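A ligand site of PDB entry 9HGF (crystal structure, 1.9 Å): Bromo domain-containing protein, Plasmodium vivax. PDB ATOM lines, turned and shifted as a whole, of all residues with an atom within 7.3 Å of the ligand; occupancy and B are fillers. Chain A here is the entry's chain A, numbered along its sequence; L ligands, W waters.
N2 of the ligand sits at hydrogen-bond distance from O of Ile 25, 2.8 Å away.
The side-chain amide nitrogen of Asn 83 lies within hydrogen-bond range of an oxygen (O2) of the ligand (3.0 Å).
O of Cys 79 sits at hydrogen-bond distance from ND2 of Asn 83, 2.9 Å away.
SG of Cys 79 is in hydrogen-bond range of O of Val 89 (3.5 Å).
The side-chain amide oxygen (OE1) of Gln 35 sits at hydrogen-bond distance from the backbone NH (N) of Asp 31.
The backbone carbonyl oxygen of Gln 35 is in hydrogen-bond range of the side-chain sulfur of Cys 37 (3.5 Å).
Phe 26 touches the ligand (CE1 to C6, 3.5 Å).
Lys 28 touches the ligand.
Val 30 touches the ligand.
CG of Gln 35 touches C3 of the ligand (3.6 Å).
Tyr 40 touches the ligand.
Tyr 82 touches the ligand (CD2 to C18, 3.7 Å).
Val 89 touches the ligand (CG2 to C10, 3.8 Å).
Hydrophobic or aromatic side chains within 4 Å of the ligand: Ile 25, Phe 26, Val 30, Tyr 40, Tyr 82 and Val 89.
Of the 24 residues printed, 9 come within 4 Å of the ligand.
The nearest printed residue that does not touch the ligand is His 24 (4.1 Å).
Water W2 bridges the side-chain hydroxyl (OH) of Tyr 40 (2.5 Å) and an oxygen (O2) of the ligand (2.9 Å).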
ATOM      1  N   HIS A  24       8.778  -0.277  21.399  1.00  0.00           N
ATOM      2  CA  HIS A  24       9.387  -1.378  20.667  1.00  0.00           C
ATOM      3  C   HIS A  24       8.403  -2.055  19.739  1.00  0.00           C
ATOM      4  O   HIS A  24       8.820  -2.691  18.765  1.00  0.00           O
ATOM      5  CB  HIS A  24       9.968  -2.426  21.627  1.00  0.00           C
ATOM      6  CG  HIS A  24       8.927  -3.065  22.496  1.00  0.00           C
ATOM      7  ND1 HIS A  24       8.449  -2.461  23.639  1.00  0.00           N
ATOM      8  CD2 HIS A  24       8.267  -4.245  22.391  1.00  0.00           C
ATOM      9  CE1 HIS A  24       7.527  -3.232  24.195  1.00  0.00           C
ATOM     10  NE2 HIS A  24       7.384  -4.316  23.449  1.00  0.00           N
ATOM     11  N   ILE A  25       7.105  -1.972  20.029  1.00  0.00           N
ATOM     12  CA  ILE A  25       6.149  -2.624  19.135  1.00  0.00           C
ATOM     13  C   ILE A  25       6.102  -1.939  17.797  1.00  0.00           C
ATOM     14  O   ILE A  25       5.593  -2.542  16.837  1.00  0.00           O
ATOM     15  CB  ILE A  25       4.743  -2.730  19.762  1.00  0.00           C
ATOM     16  CG1 ILE A  25       3.983  -1.400  19.810  1.00  0.00           C
ATOM     17  CG2 ILE A  25       4.881  -3.357  21.168  1.00  0.00           C
ATOM     18  CD1 ILE A  25       2.436  -1.584  20.273  1.00  0.00           C
ATOM     19  N   PHE A  26       6.585  -0.708  17.700  1.00  0.00           N
ATOM     20  CA  PHE A  26       6.576   0.021  16.422  1.00  0.00           C
ATOM     21  C   PHE A  26       7.928   0.040  15.730  1.00  0.00           C
ATOM     22  O   PHE A  26       8.025   0.629  14.631  1.00  0.00           O
ATOM     23  CB  PHE A  26       6.117   1.456  16.616  1.00  0.00           C
ATOM     24  CG  PHE A  26       4.702   1.545  17.156  1.00  0.00           C
ATOM     25  CD1 PHE A  26       3.672   0.947  16.468  1.00  0.00           C
ATOM     26  CD2 PHE A  26       4.430   2.174  18.375  1.00  0.00           C
ATOM     27  CE1 PHE A  26       2.333   0.982  16.993  1.00  0.00           C
ATOM     28  CE2 PHE A  26       3.076   2.231  18.886  1.00  0.00           C
ATOM     29  CZ  PHE A  26       2.066   1.630  18.201  1.00  0.00           C
ATOM     30  N   GLU A  27       8.940  -0.605  16.321  1.00  0.00           N
ATOM     31  CA  GLU A  27      10.303  -0.473  15.807  1.00  0.00           C
ATOM     32  C   GLU A  27      10.457  -1.179  14.477  1.00  0.00           C
ATOM     33  O   GLU A  27      11.017  -0.617  13.531  1.00  0.00           O
ATOM     34  CB  GLU A  27      11.316  -1.023  16.836  1.00  0.00           C
ATOM     35  CG  GLU A  27      12.794  -0.657  16.466  1.00  0.00           C
ATOM     36  CD  GLU A  27      13.040   0.860  16.462  1.00  0.00           C
ATOM     37  OE1 GLU A  27      12.382   1.558  17.261  1.00  0.00           O
ATOM     38  OE2 GLU A  27      13.871   1.374  15.646  1.00  0.00           O
ATOM     39  N   LYS A  28      10.015  -2.436  14.402  1.00  0.00           N
ATOM     40  CA  LYS A  28      10.092  -3.262  13.196  1.00  0.00           C
ATOM     41  C   LYS A  28       8.704  -3.500  12.604  1.00  0.00           C
ATOM     42  O   LYS A  28       7.709  -3.433  13.313  1.00  0.00           O
ATOM     43  CB  LYS A  28      10.734  -4.611  13.513  1.00  0.00           C
ATOM     44  CG  LYS A  28      12.086  -4.475  14.178  1.00  0.00           C
ATOM     45  CD  LYS A  28      13.047  -3.624  13.299  1.00  0.00           C
ATOM     46  CE  LYS A  28      14.495  -3.708  13.854  1.00  0.00           C
ATOM     47  NZ  LYS A  28      15.456  -2.746  13.233  1.00  0.00           N
ATOM     48  N   LEU A  29       8.650  -3.795  11.294  1.00  0.00           N
ATOM     49  CA  LEU A  29       7.366  -4.156  10.700  1.00  0.00           C
ATOM     50  C   LEU A  29       6.847  -5.450  11.322  1.00  0.00           C
ATOM     51  O   LEU A  29       7.615  -6.327  11.739  1.00  0.00           O
ATOM     52  CB  LEU A  29       7.483  -4.332   9.180  1.00  0.00           C
ATOM     53  CG  LEU A  29       7.807  -3.069   8.398  1.00  0.00           C
ATOM     54  CD1 LEU A  29       8.467  -3.416   7.047  1.00  0.00           C
ATOM     55  CD2 LEU A  29       6.515  -2.313   8.224  1.00  0.00           C
ATOM     56  N   VAL A  30       5.523  -5.542  11.405  1.00  0.00           N
ATOM     57  CA  VAL A  30       4.862  -6.734  11.912  1.00  0.00           C
ATOM     58  C   VAL A  30       5.240  -7.932  11.054  1.00  0.00           C
ATOM     59  O   VAL A  30       5.283  -7.844   9.819  1.00  0.00           O
ATOM     60  CB  VAL A  30       3.342  -6.460  11.895  1.00  0.00           C
ATOM     61  CG1 VAL A  30       2.553  -7.720  12.164  1.00  0.00           C
ATOM     62  CG2 VAL A  30       2.968  -5.397  12.934  1.00  0.00           C
ATOM     63  N   ASP A  31       5.542  -9.040  11.698  1.00  0.00           N
ATOM     64  CA  ASP A  31       5.758 -10.320  11.027  1.00  0.00           C
ATOM     65  C   ASP A  31       4.456 -11.113  11.157  1.00  0.00           C
ATOM     66  O   ASP A  31       4.060 -11.504  12.269  1.00  0.00           O
ATOM     67  CB  ASP A  31       6.959 -11.034  11.656  1.00  0.00           C
ATOM     68  CG  ASP A  31       7.304 -12.366  10.960  1.00  0.00           C
ATOM     69  OD1 ASP A  31       6.390 -13.176  10.661  1.00  0.00           O
ATOM     70  OD2 ASP A  31       8.488 -12.628  10.702  1.00  0.00           O
ATOM     71  N   LYS A  34       4.909 -14.552  12.863  1.00  0.00           N
ATOM     72  CA  LYS A  34       5.527 -14.570  14.190  1.00  0.00           C
ATOM     73  C   LYS A  34       4.680 -13.814  15.218  1.00  0.00           C
ATOM     74  O   LYS A  34       4.689 -14.162  16.393  1.00  0.00           O
ATOM     75  CB  LYS A  34       6.939 -13.975  14.085  1.00  0.00           C
ATOM     76  CG  LYS A  34       7.559 -13.575  15.403  1.00  0.00           C
ATOM     77  N   GLN A  35       3.963 -12.791  14.806  1.00  0.00           N
ATOM     78  CA  GLN A  35       3.109 -12.016  15.689  1.00  0.00           C
ATOM     79  C   GLN A  35       1.668 -12.514  15.678  1.00  0.00           C
ATOM     80  O   GLN A  35       0.773 -11.759  16.063  1.00  0.00           O
ATOM     81  CB  GLN A  35       3.154 -10.521  15.301  1.00  0.00           C
ATOM     82  CG  GLN A  35       4.159  -9.682  16.117  1.00  0.00           C
ATOM     83  CD  GLN A  35       5.590  -9.850  15.665  1.00  0.00           C
ATOM     84  OE1 GLN A  35       5.941  -9.543  14.504  1.00  0.00           O
ATOM     85  NE2 GLN A  35       6.449 -10.319  16.575  1.00  0.00           N
ATOM     86  N   ASN A  36       1.423 -13.692  15.113  1.00  0.00           N
ATOM     87  CA  ASN A  36       0.086 -14.313  15.101  1.00  0.00           C
ATOM     88  C   ASN A  36      -0.992 -13.399  14.537  1.00  0.00           C
ATOM     89  O   ASN A  36      -2.078 -13.249  15.120  1.00  0.00           O
ATOM     90  CB  ASN A  36      -0.300 -14.756  16.505  1.00  0.00           C
ATOM     91  CG  ASN A  36       0.637 -15.753  17.045  1.00  0.00           C
ATOM     92  OD1 ASN A  36       0.926 -16.744  16.374  1.00  0.00           O
ATOM     93  ND2 ASN A  36       1.174 -15.493  18.234  1.00  0.00           N
ATOM     94  N   CYS A  37      -0.698 -12.769  13.391  1.00  0.00           N
ATOM     95  CA  CYS A  37      -1.690 -11.941  12.712  1.00  0.00           C
ATOM     96  C   CYS A  37      -1.598 -12.198  11.210  1.00  0.00           C
ATOM     97  O   CYS A  37      -1.134 -11.366  10.427  1.00  0.00           O
ATOM     98  CB  CYS A  37      -1.542 -10.458  13.057  1.00  0.00           C
ATOM     99  SG  CYS A  37       0.109  -9.843  13.223  1.00  0.00           S
ATOM    100  N   TYR A  40      -2.672  -9.444   8.670  1.00  0.00           N
ATOM    101  CA  TYR A  40      -2.201  -8.067   8.872  1.00  0.00           C
ATOM    102  C   TYR A  40      -2.057  -7.309   7.552  1.00  0.00           C
ATOM    103  O   TYR A  40      -2.543  -6.175   7.416  1.00  0.00           O
ATOM    104  CB  TYR A  40      -0.874  -8.064   9.641  1.00  0.00           C
ATOM    105  CG  TYR A  40      -0.419  -6.661   9.975  1.00  0.00           C
ATOM    106  CD1 TYR A  40      -0.991  -5.958  11.025  1.00  0.00           C
ATOM    107  CD2 TYR A  40       0.550  -6.002   9.196  1.00  0.00           C
ATOM    108  CE1 TYR A  40      -0.622  -4.669  11.341  1.00  0.00           C
ATOM    109  CE2 TYR A  40       0.934  -4.704   9.497  1.00  0.00           C
ATOM    110  CZ  TYR A  40       0.364  -4.035  10.563  1.00  0.00           C
ATOM    111  OH  TYR A  40       0.741  -2.752  10.889  1.00  0.00           O
ATOM    112  N   ILE A  44      -3.607  -3.830   6.264  1.00  0.00           N
ATOM    113  CA  ILE A  44      -2.690  -2.706   6.301  1.00  0.00           C
ATOM    114  C   ILE A  44      -1.950  -2.703   4.966  1.00  0.00           C
ATOM    115  O   ILE A  44      -1.134  -3.590   4.709  1.00  0.00           O
ATOM    116  CB  ILE A  44      -1.717  -2.813   7.492  1.00  0.00           C
ATOM    117  CG1 ILE A  44      -2.461  -2.639   8.826  1.00  0.00           C
ATOM    118  CG2 ILE A  44      -0.612  -1.780   7.412  1.00  0.00           C
ATOM    119  CD1 ILE A  44      -3.513  -1.512   8.850  1.00  0.00           C
ATOM    120  N   MET A  48       4.417   0.616   7.941  1.00  0.00           N
ATOM    121  CA  MET A  48       5.411   1.599   8.352  1.00  0.00           C
ATOM    122  C   MET A  48       5.853   1.311   9.772  1.00  0.00           C
ATOM    123  O   MET A  48       5.029   0.935  10.613  1.00  0.00           O
ATOM    124  CB  MET A  48       4.868   3.021   8.269  1.00  0.00           C
ATOM    125  CG  MET A  48       5.917   4.102   8.478  1.00  0.00           C
ATOM    126  SD  MET A  48       7.163   4.100   7.105  1.00  0.00           S
ATOM    127  CE  MET A  48       6.064   4.436   5.688  1.00  0.00           C
ATOM    128  N   ILE A  75       2.082   5.110  10.961  1.00  0.00           N
ATOM    129  CA  ILE A  75       2.248   4.039  11.940  1.00  0.00           C
ATOM    130  C   ILE A  75       1.061   4.022  12.899  1.00  0.00           C
ATOM    131  O   ILE A  75       0.454   2.967  13.179  1.00  0.00           O
ATOM    132  CB  ILE A  75       3.571   4.211  12.703  1.00  0.00           C
ATOM    133  CG1 ILE A  75       4.765   4.276  11.740  1.00  0.00           C
ATOM    134  CG2 ILE A  75       3.793   3.062  13.708  1.00  0.00           C
ATOM    135  CD1 ILE A  75       6.090   4.556  12.461  1.00  0.00           C
ATOM    136  N   ASN A  78      -2.232   3.043  11.110  1.00  0.00           N
ATOM    137  CA  ASN A  78      -2.263   1.602  10.914  1.00  0.00           C
ATOM    138  C   ASN A  78      -2.639   0.910  12.206  1.00  0.00           C
ATOM    139  O   ASN A  78      -3.446  -0.039  12.218  1.00  0.00           O
ATOM    140  CB  ASN A  78      -0.911   1.080  10.433  1.00  0.00           C
ATOM    141  CG  ASN A  78      -0.614   1.510   8.999  1.00  0.00           C
ATOM    142  OD1 ASN A  78      -1.507   1.971   8.314  1.00  0.00           O
ATOM    143  ND2 ASN A  78       0.645   1.352   8.548  1.00  0.00           N
ATOM    144  N   CYS A  79      -2.039   1.365  13.302  1.00  0.00           N
ATOM    145  CA  CYS A  79      -2.298   0.796  14.613  1.00  0.00           C
ATOM    146  C   CYS A  79      -3.782   0.845  14.958  1.00  0.00           C
ATOM    147  O   CYS A  79      -4.385  -0.168  15.324  1.00  0.00           O
ATOM    148  CB  CYS A  79      -1.492   1.546  15.650  1.00  0.00           C
ATOM    149  SG  CYS A  79      -1.616   0.794  17.323  1.00  0.00           S
ATOM    150  N   SER A  80      -4.398   2.034  14.860  1.00  0.00           N
ATOM    151  CA  SER A  80      -5.808   2.155  15.253  1.00  0.00           C
ATOM    152  C   SER A  80      -6.736   1.462  14.269  1.00  0.00           C
ATOM    153  O   SER A  80      -7.838   1.013  14.643  1.00  0.00           O
ATOM    154  CB  SER A  80      -6.183   3.620  15.391  1.00  0.00           C
ATOM    155  OG  SER A  80      -5.976   4.270  14.163  1.00  0.00           O
ATOM    156  N   TYR A  82      -5.962  -1.525  12.536  1.00  0.00           N
ATOM    157  CA  TYR A  82      -5.918  -2.971  12.724  1.00  0.00           C
ATOM    158  C   TYR A  82      -6.360  -3.383  14.122  1.00  0.00           C
ATOM    159  O   TYR A  82      -6.961  -4.446  14.281  1.00  0.00           O
ATOM    160  CB  TYR A  82      -4.499  -3.514  12.461  1.00  0.00           C
ATOM    161  CG  TYR A  82      -4.448  -5.044  12.516  1.00  0.00           C
ATOM    162  CD1 TYR A  82      -4.816  -5.802  11.413  1.00  0.00           C
ATOM    163  CD2 TYR A  82      -4.078  -5.716  13.689  1.00  0.00           C
ATOM    164  CE1 TYR A  82      -4.791  -7.185  11.443  1.00  0.00           C
ATOM    165  CE2 TYR A  82      -4.067  -7.117  13.729  1.00  0.00           C
ATOM    166  CZ  TYR A  82      -4.434  -7.831  12.593  1.00  0.00           C
ATOM    167  OH  TYR A  82      -4.455  -9.206  12.594  1.00  0.00           O
ATOM    168  N   ASN A  83      -6.048  -2.589  15.151  1.00  0.00           N
ATOM    169  CA  ASN A  83      -6.188  -3.062  16.524  1.00  0.00           C
ATOM    170  C   ASN A  83      -7.461  -2.533  17.160  1.00  0.00           C
ATOM    171  O   ASN A  83      -7.887  -1.404  16.893  1.00  0.00           O
ATOM    172  CB  ASN A  83      -4.980  -2.679  17.375  1.00  0.00           C
ATOM    173  CG  ASN A  83      -3.726  -3.327  16.878  1.00  0.00           C
ATOM    174  OD1 ASN A  83      -3.459  -4.482  17.164  1.00  0.00           O
ATOM    175  ND2 ASN A  83      -2.981  -2.599  16.028  1.00  0.00           N
ATOM    176  N   LEU A  88      -4.091  -3.583  24.261  1.00  0.00           N
ATOM    177  CA  LEU A  88      -2.797  -3.079  24.717  1.00  0.00           C
ATOM    178  C   LEU A  88      -2.072  -2.383  23.557  1.00  0.00           C
ATOM    179  O   LEU A  88      -1.451  -1.336  23.727  1.00  0.00           O
ATOM    180  CB  LEU A  88      -1.929  -4.206  25.245  1.00  0.00           C
ATOM    181  CG  LEU A  88      -2.431  -4.939  26.519  1.00  0.00           C
ATOM    182  CD1 LEU A  88      -1.289  -5.787  27.066  1.00  0.00           C
ATOM    183  CD2 LEU A  88      -2.934  -3.938  27.538  1.00  0.00           C
ATOM    184  N   VAL A  89      -2.194  -2.957  22.361  1.00  0.00           N
ATOM    185  CA  VAL A  89      -1.469  -2.355  21.240  1.00  0.00           C
ATOM    186  C   VAL A  89      -2.104  -1.003  20.878  1.00  0.00           C
ATOM    187  O   VAL A  89      -1.397  -0.002  20.696  1.00  0.00           O
ATOM    188  CB  VAL A  89      -1.416  -3.328  20.047  1.00  0.00           C
ATOM    189  CG1 VAL A  89      -0.869  -2.642  18.767  1.00  0.00           C
ATOM    190  CG2 VAL A  89      -0.545  -4.523  20.416  1.00  0.00           C
ATOM    191  N   ALA A  90      -3.442  -0.936  20.875  1.00  0.00           N
ATOM    192  CA  ALA A  90      -4.099   0.313  20.493  1.00  0.00           C
ATOM    193  C   ALA A  90      -3.844   1.405  21.521  1.00  0.00           C
ATOM    194  O   ALA A  90      -3.628   2.574  21.169  1.00  0.00           O
ATOM    195  CB  ALA A  90      -5.612   0.109  20.297  1.00  0.00           C
HETATM  196  C1  LIG L   1       2.010  -5.934  16.588  1.00  0.00           C
HETATM  197  C2  LIG L   1       1.359  -4.780  15.997  1.00  0.00           C
HETATM  198  C3  LIG L   1       1.444  -7.353  16.636  1.00  0.00           C
HETATM  199  C4  LIG L   1       0.021  -7.516  17.319  1.00  0.00           C
HETATM  200  C5  LIG L   1      -1.133  -6.835  16.550  1.00  0.00           C
HETATM  201  C6  LIG L   1       1.978  -2.228  15.690  1.00  0.00           C
HETATM  202  C7  LIG L   1       4.341  -6.058  17.758  1.00  0.00           C
HETATM  203  C8  LIG L   1       3.259  -5.448  17.058  1.00  0.00           C
HETATM  204  C9  LIG L   1       5.748  -5.720  15.568  1.00  0.00           C
HETATM  205  C10 LIG L   1       2.793  -6.274  19.857  1.00  0.00           C
HETATM  206  C11 LIG L   1       4.163  -6.444  19.127  1.00  0.00           C
HETATM  207  C12 LIG L   1       5.283  -6.992  19.778  1.00  0.00           C
HETATM  208  C13 LIG L   1       6.526  -7.132  19.108  1.00  0.00           C
HETATM  209  C14 LIG L   1       7.755  -7.705  19.829  1.00  0.00           C
HETATM  210  C15 LIG L   1       6.655  -6.719  17.755  1.00  0.00           C
HETATM  211  C16 LIG L   1       5.596  -6.157  17.056  1.00  0.00           C
HETATM  212  C17 LIG L   1       2.180  -3.661  16.127  1.00  0.00           C
HETATM  213  C18 LIG L   1      -0.744  -6.180  15.202  1.00  0.00           C
HETATM  214  C19 LIG L   1       0.016  -4.897  15.357  1.00  0.00           C
HETATM  215  N1  LIG L   1       8.998  -7.872  19.202  1.00  0.00           N
HETATM  216  N2  LIG L   1       3.298  -4.090  16.777  1.00  0.00           N
HETATM  217  O1  LIG L   1       7.651  -8.035  21.023  1.00  0.00           O
HETATM  218  O2  LIG L   1      -0.489  -3.842  14.931  1.00  0.00           O
HETATM  219  O   HOH W   1       9.872  -6.861  15.968  1.00  0.00           O
HETATM  220  O   HOH W   2      -0.346  -1.823  12.881  1.00  0.00           O
